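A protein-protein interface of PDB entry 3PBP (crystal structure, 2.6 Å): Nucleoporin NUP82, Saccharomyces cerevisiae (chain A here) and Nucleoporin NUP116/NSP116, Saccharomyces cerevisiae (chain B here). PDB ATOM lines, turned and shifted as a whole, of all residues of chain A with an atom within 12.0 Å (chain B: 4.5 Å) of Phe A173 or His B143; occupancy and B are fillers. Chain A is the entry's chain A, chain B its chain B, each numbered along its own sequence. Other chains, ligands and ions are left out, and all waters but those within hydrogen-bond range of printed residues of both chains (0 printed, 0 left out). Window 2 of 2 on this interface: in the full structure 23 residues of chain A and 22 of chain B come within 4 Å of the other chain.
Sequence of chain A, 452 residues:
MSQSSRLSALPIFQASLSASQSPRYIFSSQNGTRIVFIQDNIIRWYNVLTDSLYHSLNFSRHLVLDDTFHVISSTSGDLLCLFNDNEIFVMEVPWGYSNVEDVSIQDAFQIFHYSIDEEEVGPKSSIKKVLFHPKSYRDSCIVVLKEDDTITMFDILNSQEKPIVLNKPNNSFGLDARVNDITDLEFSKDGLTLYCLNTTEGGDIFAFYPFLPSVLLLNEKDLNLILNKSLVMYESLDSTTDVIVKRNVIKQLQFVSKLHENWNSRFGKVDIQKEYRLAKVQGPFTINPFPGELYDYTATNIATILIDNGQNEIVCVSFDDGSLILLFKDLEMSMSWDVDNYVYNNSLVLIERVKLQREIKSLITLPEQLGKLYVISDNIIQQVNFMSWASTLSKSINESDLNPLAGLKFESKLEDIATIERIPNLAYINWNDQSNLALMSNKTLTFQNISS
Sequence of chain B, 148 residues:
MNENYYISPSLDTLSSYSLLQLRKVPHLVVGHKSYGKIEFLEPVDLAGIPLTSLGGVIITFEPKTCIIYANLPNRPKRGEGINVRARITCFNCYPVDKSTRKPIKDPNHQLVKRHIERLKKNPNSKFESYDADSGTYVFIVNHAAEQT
OG1 of Thr B65 sits at hydrogen-bond distance from O of Leu A175 (3.4 Å).
The backbone NH (N) of Leu A175 lies within hydrogen-bond range of the backbone carbonyl oxygen (O) of Lys B64, 2.9 Å away.
The backbone NH (N) of Phe A173 is in hydrogen-bond range of the backbone carbonyl oxygen (O) of Cys B66 (3.1 Å).
OE2 of Glu B146 sits at hydrogen-bond distance from ND2 of Asn B83 (3.3 Å).
The backbone carbonyl oxygen of Val B84 sits at hydrogen-bond distance from the backbone NH of Ala B144 (3.0 Å).
The guanidinium group of Arg B78 lies within salt-bridge range of the side-chain carboxylate of Glu B146 (2.9 Å).
The backbone NH (N) of Ile B88 is in hydrogen-bond range of the backbone carbonyl oxygen (O) of Phe B139 (2.9 Å).
Among the printed residues, merely in contact across the chains: Ser A172 with Thr B65 (3.8 Å), Ser A172 with Cys B66 (3.6 Å), Phe A173 with Thr B65 (3.5 Å), Phe A173 with Ile B68 (3.96 Å), Phe A173 with Ile B88 (3.3 Å), Phe A173 with Phe B139 (3.7 Å), Phe A173 with Val B141 (3.8 Å), Phe A173 with His B143 (3.7 Å), Phe A173 with Ala B144 (2.9 Å), Phe A173 with Glu B146 (3.8 Å), Gly A174 with Lys B64 (3.3 Å) and Gly A174 with Phe B139 (3.5 Å).
Of the printed residues of chain B, Phe A173 touches Thr B65, Cys B66, Ile B68, Ile B88, Phe B139, Val B141, His B143, Ala B144 and Glu B146.
His B143 touches just one residue of chain A: Phe A173 (3.7 Å).
Thr B65 touches three residues of chain A.
Of chain A, only Ser A172 and Phe A173 come within 4 Å of Cys B66.
No residue of chain A comes within 4 Å of Arg B78.
No residue of chain A comes within 4 Å of Val B84.
Printed residues of chain A within 4 Å of Ile B88: Phe A173 (3.3 Å).
Asn B124 touches none of the printed residues of chain A.
Of chain A, only Phe A173 (3.8 Å) comes within 4 Å of Val B141.
No residue of chain A comes within 4 Å of Asn B142.
Ala B144 touches one residue of chain A.
Printed residues of chain A within 4 Å of Glu B146: Phe A173 (3.8 Å).
Of the printed residues of chain B, Leu A175 touches Lys B64 and Thr B65.
Of the printed residues of chain A, Ile B68 touches Phe A173 (3.96 Å).
Printed residues of chain B within 4 Å of Ser A172: Thr B65 (3.8 Å) and Cys B66 (3.6 Å).
Of the printed residues of chain A, Phe B139 touches Phe A173 (3.7 Å) and Gly A174 (3.5 Å).
Printed residues of chain A within 4 Å of Lys B64: Gly A174 (3.3 Å) and Leu A175 (2.9 Å).
Ala A177 touches none of the printed residues of chain B.
Asn A170 touches none of the printed residues of chain B.
The nearest residue of chain A that does not touch His B143 is Asn A171 (8.1 Å).
The nearest printed residue of chain B that does not touch Ser A172 is Ile B68 (5.7 Å).
Of the 15 printed residues of chain A, 4 touch a printed residue of chain B.
Hydrophobic or aromatic side chains of chain A that line the printed part of chain B: Phe A173.
Of the 16 printed residues of chain B, 10 touch a printed residue of chain A.
Hydrophobic or aromatic side chains of chain B that line the printed part of chain A: Ile B68, Ile B88, Phe B139 and Val B141.
Among the printed residues, 15 pairs touch across the chains.
Among the printed residues, no Asp or Glu carboxylate lies within 4 Å of a Lys or Arg side-chain nitrogen of the other chain.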
ATOM      1  N   LYS A 168      -8.209 -27.949  17.957  1.00  0.00           N
ATOM      2  CA  LYS A 168      -9.456 -27.202  17.846  1.00  0.00           C
ATOM      3  C   LYS A 168      -9.340 -25.871  18.574  1.00  0.00           C
ATOM      4  O   LYS A 168      -8.562 -25.734  19.529  1.00  0.00           O
ATOM      5  CB  LYS A 168     -10.608 -27.997  18.456  1.00  0.00           C
ATOM      6  CG  LYS A 168     -10.854 -29.352  17.832  1.00  0.00           C
ATOM      7  CD  LYS A 168     -11.958 -30.077  18.579  1.00  0.00           C
ATOM      8  CE  LYS A 168     -11.998 -31.561  18.232  1.00  0.00           C
ATOM      9  NZ  LYS A 168     -12.885 -32.339  19.153  1.00  0.00           N
ATOM     10  N   PRO A 169     -10.108 -24.862  18.131  1.00  0.00           N
ATOM     11  CA  PRO A 169     -10.041 -23.559  18.796  1.00  0.00           C
ATOM     12  C   PRO A 169     -10.514 -23.650  20.251  1.00  0.00           C
ATOM     13  O   PRO A 169     -11.322 -24.515  20.603  1.00  0.00           O
ATOM     14  CB  PRO A 169     -10.949 -22.687  17.932  1.00  0.00           C
ATOM     15  CG  PRO A 169     -10.826 -23.308  16.571  1.00  0.00           C
ATOM     16  CD  PRO A 169     -10.898 -24.780  16.892  1.00  0.00           C
ATOM     17  N   ASN A 170      -9.992 -22.758  21.088  1.00  0.00           N
ATOM     18  CA  ASN A 170     -10.348 -22.714  22.502  1.00  0.00           C
ATOM     19  C   ASN A 170     -11.131 -21.465  22.871  1.00  0.00           C
ATOM     20  O   ASN A 170     -11.185 -20.489  22.112  1.00  0.00           O
ATOM     21  CB  ASN A 170      -9.096 -22.752  23.379  1.00  0.00           C
ATOM     22  CG  ASN A 170      -8.541 -24.146  23.541  1.00  0.00           C
ATOM     23  OD1 ASN A 170      -9.250 -25.062  23.964  1.00  0.00           O
ATOM     24  ND2 ASN A 170      -7.259 -24.318  23.214  1.00  0.00           N
ATOM     25  N   ASN A 171     -11.736 -21.522  24.054  1.00  0.00           N
ATOM     26  CA  ASN A 171     -12.500 -20.415  24.609  1.00  0.00           C
ATOM     27  C   ASN A 171     -11.662 -19.908  25.754  1.00  0.00           C
ATOM     28  O   ASN A 171     -12.148 -19.740  26.871  1.00  0.00           O
ATOM     29  CB  ASN A 171     -13.858 -20.886  25.135  1.00  0.00           C
ATOM     30  CG  ASN A 171     -14.878 -21.055  24.028  1.00  0.00           C
ATOM     31  OD1 ASN A 171     -15.250 -20.082  23.357  1.00  0.00           O
ATOM     32  ND2 ASN A 171     -15.330 -22.291  23.818  1.00  0.00           N
ATOM     33  N   SER A 172     -10.383 -19.700  25.471  1.00  0.00           N
ATOM     34  CA  SER A 172      -9.456 -19.215  26.472  1.00  0.00           C
ATOM     35  C   SER A 172      -9.024 -17.812  26.119  1.00  0.00           C
ATOM     36  O   SER A 172      -9.245 -17.342  25.005  1.00  0.00           O
ATOM     37  CB  SER A 172      -8.219 -20.109  26.538  1.00  0.00           C
ATOM     38  OG  SER A 172      -8.545 -21.407  26.984  1.00  0.00           O
ATOM     39  N   PHE A 173      -8.429 -17.143  27.093  1.00  0.00           N
ATOM     40  CA  PHE A 173      -7.906 -15.806  26.914  1.00  0.00           C
ATOM     41  C   PHE A 173      -6.480 -15.966  27.410  1.00  0.00           C
ATOM     42  O   PHE A 173      -6.158 -16.973  28.036  1.00  0.00           O
ATOM     43  CB  PHE A 173      -8.661 -14.793  27.781  1.00  0.00           C
ATOM     44  CG  PHE A 173     -10.077 -14.538  27.338  1.00  0.00           C
ATOM     45  CD1 PHE A 173     -10.354 -14.151  26.031  1.00  0.00           C
ATOM     46  CD2 PHE A 173     -11.133 -14.656  28.238  1.00  0.00           C
ATOM     47  CE1 PHE A 173     -11.665 -13.886  25.628  1.00  0.00           C
ATOM     48  CE2 PHE A 173     -12.443 -14.391  27.842  1.00  0.00           C
ATOM     49  CZ  PHE A 173     -12.709 -14.006  26.536  1.00  0.00           C
ATOM     50  N   GLY A 174      -5.622 -14.995  27.133  1.00  0.00           N
ATOM     51  CA  GLY A 174      -4.251 -15.111  27.587  1.00  0.00           C
ATOM     52  C   GLY A 174      -3.403 -15.859  26.584  1.00  0.00           C
ATOM     53  O   GLY A 174      -3.889 -16.274  25.528  1.00  0.00           O
ATOM     54  N   LEU A 175      -2.137 -16.058  26.934  1.00  0.00           N
ATOM     55  CA  LEU A 175      -1.190 -16.720  26.050  1.00  0.00           C
ATOM     56  C   LEU A 175      -1.191 -18.267  26.011  1.00  0.00           C
ATOM     57  O   LEU A 175      -1.428 -18.950  27.015  1.00  0.00           O
ATOM     58  CB  LEU A 175       0.225 -16.212  26.377  1.00  0.00           C
ATOM     59  CG  LEU A 175       0.398 -14.704  26.596  1.00  0.00           C
ATOM     60  CD1 LEU A 175       1.835 -14.400  27.017  1.00  0.00           C
ATOM     61  CD2 LEU A 175       0.037 -13.963  25.327  1.00  0.00           C
ATOM     62  N   ASP A 176      -0.934 -18.787  24.810  1.00  0.00           N
ATOM     63  CA  ASP A 176      -0.816 -20.217  24.519  1.00  0.00           C
ATOM     64  C   ASP A 176      -1.928 -21.187  24.930  1.00  0.00           C
ATOM     65  O   ASP A 176      -1.657 -22.191  25.592  1.00  0.00           O
ATOM     66  CB  ASP A 176       0.515 -20.732  25.083  1.00  0.00           C
ATOM     67  CG  ASP A 176       1.624 -19.689  25.016  1.00  0.00           C
ATOM     68  OD1 ASP A 176       1.818 -19.082  23.937  1.00  0.00           O
ATOM     69  OD2 ASP A 176       2.304 -19.486  26.050  1.00  0.00           O
ATOM     70  N   ALA A 177      -3.164 -20.915  24.532  1.00  0.00           N
ATOM     71  CA  ALA A 177      -4.248 -21.838  24.856  1.00  0.00           C
ATOM     72  C   ALA A 177      -3.941 -23.154  24.123  1.00  0.00           C
ATOM     73  O   ALA A 177      -3.951 -24.242  24.715  1.00  0.00           O
ATOM     74  CB  ALA A 177      -5.584 -21.267  24.389  1.00  0.00           C
ATOM     75  N   ARG A 178      -3.655 -23.026  22.826  1.00  0.00           N
ATOM     76  CA  ARG A 178      -3.305 -24.144  21.934  1.00  0.00           C
ATOM     77  C   ARG A 178      -2.307 -23.560  20.913  1.00  0.00           C
ATOM     78  O   ARG A 178      -1.970 -22.366  20.986  1.00  0.00           O
ATOM     79  CB  ARG A 178      -4.546 -24.643  21.196  1.00  0.00           C
ATOM     80  CG  ARG A 178      -5.280 -23.494  20.516  1.00  0.00           C
ATOM     81  CD  ARG A 178      -6.056 -23.919  19.298  1.00  0.00           C
ATOM     82  NE  ARG A 178      -6.252 -22.773  18.416  1.00  0.00           N
ATOM     83  CZ  ARG A 178      -6.686 -22.856  17.166  1.00  0.00           C
ATOM     84  NH1 ARG A 178      -6.980 -24.035  16.641  1.00  0.00           N
ATOM     85  NH2 ARG A 178      -6.805 -21.759  16.437  1.00  0.00           N
ATOM     86  N   VAL A 179      -1.847 -24.370  19.959  1.00  0.00           N
ATOM     87  CA  VAL A 179      -0.894 -23.867  18.969  1.00  0.00           C
ATOM     88  C   VAL A 179      -1.552 -22.980  17.913  1.00  0.00           C
ATOM     89  O   VAL A 179      -2.447 -23.419  17.192  1.00  0.00           O
ATOM     90  CB  VAL A 179      -0.169 -25.007  18.246  1.00  0.00           C
ATOM     91  CG1 VAL A 179       0.968 -24.446  17.412  1.00  0.00           C
ATOM     92  CG2 VAL A 179       0.343 -26.002  19.245  1.00  0.00           C
ATOM     93  N   ASN A 180      -1.088 -21.738  17.820  1.00  0.00           N
ATOM     94  CA  ASN A 180      -1.615 -20.774  16.861  1.00  0.00           C
ATOM     95  C   ASN A 180      -0.545 -20.317  15.892  1.00  0.00           C
ATOM     96  O   ASN A 180       0.646 -20.468  16.153  1.00  0.00           O
ATOM     97  CB  ASN A 180      -2.173 -19.552  17.593  1.00  0.00           C
ATOM     98  CG  ASN A 180      -3.446 -19.866  18.364  1.00  0.00           C
ATOM     99  OD1 ASN A 180      -4.523 -19.999  17.769  1.00  0.00           O
ATOM    100  ND2 ASN A 180      -3.331 -20.005  19.690  1.00  0.00           N
ATOM    101  N   THR A 200       3.644 -17.457  16.336  1.00  0.00           N
ATOM    102  CA  THR A 200       3.257 -16.640  17.485  1.00  0.00           C
ATOM    103  C   THR A 200       4.403 -15.851  18.138  1.00  0.00           C
ATOM    104  O   THR A 200       4.239 -14.678  18.468  1.00  0.00           O
ATOM    105  CB  THR A 200       2.598 -17.495  18.583  1.00  0.00           C
ATOM    106  OG1 THR A 200       1.568 -18.308  18.006  1.00  0.00           O
ATOM    107  CG2 THR A 200       1.996 -16.600  19.657  1.00  0.00           C
ATOM    108  N   ASN A 341      -0.394 -28.591  27.116  1.00  0.00           N
ATOM    109  CA  ASN A 341       0.941 -28.035  27.266  1.00  0.00           C
ATOM    110  C   ASN A 341       1.954 -29.055  27.761  1.00  0.00           C
ATOM    111  O   ASN A 341       2.854 -28.735  28.541  1.00  0.00           O
ATOM    112  CB  ASN A 341       0.882 -26.850  28.209  1.00  0.00           C
ATOM    113  CG  ASN A 341      -0.102 -25.819  27.739  1.00  0.00           C
ATOM    114  OD1 ASN A 341       0.097 -25.192  26.693  1.00  0.00           O
ATOM    115  ND2 ASN A 341      -1.195 -25.649  28.489  1.00  0.00           N
ATOM    116  N   LYS B  64      -0.700 -18.308  32.619  1.00  0.00           N
ATOM    117  CA  LYS B  64      -0.898 -17.530  31.398  1.00  0.00           C
ATOM    118  C   LYS B  64      -2.265 -17.652  30.716  1.00  0.00           C
ATOM    119  O   LYS B  64      -2.492 -17.025  29.680  1.00  0.00           O
ATOM    120  CB  LYS B  64       0.201 -17.872  30.386  1.00  0.00           C
ATOM    121  CG  LYS B  64       1.619 -17.584  30.864  1.00  0.00           C
ATOM    122  CD  LYS B  64       2.642 -17.939  29.790  1.00  0.00           C
ATOM    123  CE  LYS B  64       4.059 -17.596  30.232  1.00  0.00           C
ATOM    124  NZ  LYS B  64       5.077 -17.908  29.190  1.00  0.00           N
ATOM    125  N   THR B  65      -3.175 -18.436  31.288  1.00  0.00           N
ATOM    126  CA  THR B  65      -4.495 -18.625  30.685  1.00  0.00           C
ATOM    127  C   THR B  65      -5.662 -18.332  31.618  1.00  0.00           C
ATOM    128  O   THR B  65      -5.542 -18.445  32.830  1.00  0.00           O
ATOM    129  CB  THR B  65      -4.652 -20.073  30.148  1.00  0.00           C
ATOM    130  OG1 THR B  65      -3.721 -20.294  29.085  1.00  0.00           O
ATOM    131  CG2 THR B  65      -6.058 -20.310  29.620  1.00  0.00           C
ATOM    132  N   CYS B  66      -6.791 -17.953  31.028  1.00  0.00           N
ATOM    133  CA  CYS B  66      -8.020 -17.660  31.760  1.00  0.00           C
ATOM    134  C   CYS B  66      -9.163 -18.311  30.987  1.00  0.00           C
ATOM    135  O   CYS B  66      -9.466 -17.912  29.870  1.00  0.00           O
ATOM    136  CB  CYS B  66      -8.245 -16.152  31.848  1.00  0.00           C
ATOM    137  SG  CYS B  66      -9.888 -15.684  32.427  1.00  0.00           S
ATOM    138  N   ILE B  68     -13.182 -19.281  30.728  1.00  0.00           N
ATOM    139  CA  ILE B  68     -14.514 -18.994  31.231  1.00  0.00           C
ATOM    140  C   ILE B  68     -15.510 -20.030  30.718  1.00  0.00           C
ATOM    141  O   ILE B  68     -15.556 -20.323  29.526  1.00  0.00           O
ATOM    142  CB  ILE B  68     -14.960 -17.569  30.828  1.00  0.00           C
ATOM    143  CG1 ILE B  68     -14.054 -16.544  31.517  1.00  0.00           C
ATOM    144  CG2 ILE B  68     -16.416 -17.334  31.219  1.00  0.00           C
ATOM    145  CD1 ILE B  68     -14.400 -15.109  31.214  1.00  0.00           C
ATOM    146  N   ARG B  78     -24.549 -12.252  24.113  1.00  0.00           N
ATOM    147  CA  ARG B  78     -23.848 -11.014  24.424  1.00  0.00           C
ATOM    148  C   ARG B  78     -24.636 -10.076  25.331  1.00  0.00           C
ATOM    149  O   ARG B  78     -25.807  -9.794  25.087  1.00  0.00           O
ATOM    150  CB  ARG B  78     -23.460 -10.309  23.129  1.00  0.00           C
ATOM    151  CG  ARG B  78     -22.416 -11.081  22.369  1.00  0.00           C
ATOM    152  CD  ARG B  78     -22.094 -10.478  21.036  1.00  0.00           C
ATOM    153  NE  ARG B  78     -20.969 -11.180  20.431  1.00  0.00           N
ATOM    154  CZ  ARG B  78     -20.490 -10.930  19.219  1.00  0.00           C
ATOM    155  NH1 ARG B  78     -21.042  -9.987  18.465  1.00  0.00           N
ATOM    156  NH2 ARG B  78     -19.455 -11.623  18.759  1.00  0.00           N
ATOM    157  N   ASN B  83     -21.442 -12.814  29.958  1.00  0.00           N
ATOM    158  CA  ASN B  83     -20.881 -12.456  28.652  1.00  0.00           C
ATOM    159  C   ASN B  83     -20.954 -10.938  28.460  1.00  0.00           C
ATOM    160  O   ASN B  83     -21.861 -10.410  27.802  1.00  0.00           O
ATOM    161  CB  ASN B  83     -21.640 -13.177  27.544  1.00  0.00           C
ATOM    162  CG  ASN B  83     -20.840 -13.272  26.277  1.00  0.00           C
ATOM    163  OD1 ASN B  83     -19.616 -13.387  26.320  1.00  0.00           O
ATOM    164  ND2 ASN B  83     -21.521 -13.242  25.134  1.00  0.00           N
ATOM    165  N   VAL B  84     -19.974 -10.248  29.038  1.00  0.00           N
ATOM    166  CA  VAL B  84     -19.910  -8.797  29.018  1.00  0.00           C
ATOM    167  C   VAL B  84     -18.446  -8.328  28.947  1.00  0.00           C
ATOM    168  O   VAL B  84     -17.535  -9.136  29.122  1.00  0.00           O
ATOM    169  CB  VAL B  84     -20.617  -8.280  30.288  1.00  0.00           C
ATOM    170  CG1 VAL B  84     -19.620  -7.727  31.273  1.00  0.00           C
ATOM    171  CG2 VAL B  84     -21.679  -7.284  29.914  1.00  0.00           C
ATOM    172  N   ILE B  88      -8.952  -8.406  31.764  1.00  0.00           N
ATOM    173  CA  ILE B  88      -8.237  -9.573  32.246  1.00  0.00           C
ATOM    174  C   ILE B  88      -6.769  -9.255  32.529  1.00  0.00           C
ATOM    175  O   ILE B  88      -6.123  -8.537  31.770  1.00  0.00           O
ATOM    176  CB  ILE B  88      -8.360 -10.731  31.225  1.00  0.00           C
ATOM    177  CG1 ILE B  88      -9.830 -11.135  31.117  1.00  0.00           C
ATOM    178  CG2 ILE B  88      -7.490 -11.914  31.643  1.00  0.00           C
ATOM    179  CD1 ILE B  88     -10.085 -12.284  30.209  1.00  0.00           C
ATOM    180  N   ASN B 124      -8.049 -11.270  19.504  1.00  0.00           N
ATOM    181  CA  ASN B 124      -9.408 -11.184  20.053  1.00  0.00           C
ATOM    182  C   ASN B 124      -9.223 -10.932  21.555  1.00  0.00           C
ATOM    183  O   ASN B 124      -9.747 -11.656  22.403  1.00  0.00           O
ATOM    184  CB  ASN B 124     -10.222 -12.467  19.810  1.00  0.00           C
ATOM    185  CG  ASN B 124     -11.356 -12.265  18.787  1.00  0.00           C
ATOM    186  OD1 ASN B 124     -12.117 -11.289  18.854  1.00  0.00           O
ATOM    187  ND2 ASN B 124     -11.475 -13.198  17.844  1.00  0.00           N
ATOM    188  N   PHE B 139      -5.228  -6.883  29.345  1.00  0.00           N
ATOM    189  CA  PHE B 139      -5.948  -6.661  28.103  1.00  0.00           C
ATOM    190  C   PHE B 139      -7.457  -6.631  28.338  1.00  0.00           C
ATOM    191  O   PHE B 139      -7.929  -7.069  29.389  1.00  0.00           O
ATOM    192  CB  PHE B 139      -5.588  -7.746  27.081  1.00  0.00           C
ATOM    193  CG  PHE B 139      -5.924  -9.152  27.518  1.00  0.00           C
ATOM    194  CD1 PHE B 139      -5.020  -9.905  28.275  1.00  0.00           C
ATOM    195  CD2 PHE B 139      -7.129  -9.740  27.149  1.00  0.00           C
ATOM    196  CE1 PHE B 139      -5.309 -11.222  28.650  1.00  0.00           C
ATOM    197  CE2 PHE B 139      -7.427 -11.053  27.520  1.00  0.00           C
ATOM    198  CZ  PHE B 139      -6.514 -11.794  28.270  1.00  0.00           C
ATOM    199  N   VAL B 141     -11.437  -7.520  26.788  1.00  0.00           N
ATOM    200  CA  VAL B 141     -12.201  -8.378  25.871  1.00  0.00           C
ATOM    201  C   VAL B 141     -13.643  -7.882  25.924  1.00  0.00           C
ATOM    202  O   VAL B 141     -14.180  -7.637  26.999  1.00  0.00           O
ATOM    203  CB  VAL B 141     -12.133  -9.901  26.261  1.00  0.00           C
ATOM    204  CG1 VAL B 141     -10.685 -10.336  26.432  1.00  0.00           C
ATOM    205  CG2 VAL B 141     -12.927 -10.181  27.524  1.00  0.00           C
ATOM    206  N   ASN B 142     -14.270  -7.708  24.770  1.00  0.00           N
ATOM    207  CA  ASN B 142     -15.628  -7.193  24.761  1.00  0.00           C
ATOM    208  C   ASN B 142     -16.675  -8.142  25.303  1.00  0.00           C
ATOM    209  O   ASN B 142     -17.674  -7.700  25.851  1.00  0.00           O
ATOM    210  CB  ASN B 142     -16.019  -6.740  23.357  1.00  0.00           C
ATOM    211  CG  ASN B 142     -15.200  -5.549  22.887  1.00  0.00           C
ATOM    212  OD1 ASN B 142     -14.724  -4.748  23.697  1.00  0.00           O
ATOM    213  ND2 ASN B 142     -15.042  -5.421  21.575  1.00  0.00           N
ATOM    214  N   HIS B 143     -16.443  -9.442  25.159  1.00  0.00           N
ATOM    215  CA  HIS B 143     -17.385 -10.445  25.646  1.00  0.00           C
ATOM    216  C   HIS B 143     -16.628 -11.578  26.342  1.00  0.00           C
ATOM    217  O   HIS B 143     -15.956 -12.376  25.691  1.00  0.00           O
ATOM    218  CB  HIS B 143     -18.202 -10.983  24.473  1.00  0.00           C
ATOM    219  CG  HIS B 143     -18.930  -9.922  23.706  1.00  0.00           C
ATOM    220  ND1 HIS B 143     -20.010  -9.237  24.224  1.00  0.00           N
ATOM    221  CD2 HIS B 143     -18.722  -9.417  22.465  1.00  0.00           C
ATOM    222  CE1 HIS B 143     -20.435  -8.354  23.337  1.00  0.00           C
ATOM    223  NE2 HIS B 143     -19.671  -8.444  22.261  1.00  0.00           N
ATOM    224  N   ALA B 144     -16.745 -11.639  27.667  1.00  0.00           N
ATOM    225  CA  ALA B 144     -16.060 -12.649  28.475  1.00  0.00           C
ATOM    226  C   ALA B 144     -16.243 -14.093  27.997  1.00  0.00           C
ATOM    227  O   ALA B 144     -15.272 -14.847  27.912  1.00  0.00           O
ATOM    228  CB  ALA B 144     -16.495 -12.523  29.929  1.00  0.00           C
ATOM    229  N   ALA B 145     -17.481 -14.475  27.690  1.00  0.00           N
ATOM    230  CA  ALA B 145     -17.773 -15.835  27.233  1.00  0.00           C
ATOM    231  C   ALA B 145     -17.725 -15.983  25.708  1.00  0.00           C
ATOM    232  O   ALA B 145     -18.748 -16.197  25.058  1.00  0.00           O
ATOM    233  CB  ALA B 145     -19.134 -16.270  27.756  1.00  0.00           C
ATOM    234  N   GLU B 146     -16.522 -15.877  25.151  1.00  0.00           N
ATOM    235  CA  GLU B 146     -16.304 -15.990  23.711  1.00  0.00           C
ATOM    236  C   GLU B 146     -14.809 -16.035  23.406  1.00  0.00           C
ATOM    237  O   GLU B 146     -14.256 -14.962  23.086  1.00  0.00           O
ATOM    238  CB  GLU B 146     -16.942 -14.810  22.966  1.00  0.00           C
ATOM    239  CG  GLU B 146     -18.360 -15.071  22.481  1.00  0.00           C
ATOM    240  CD  GLU B 146     -18.965 -13.882  21.746  1.00  0.00           C
ATOM    241  OE1 GLU B 146     -18.333 -13.383  20.790  1.00  0.00           O
ATOM    242  OE2 GLU B 146     -20.078 -13.446  22.118  1.00  0.00           O
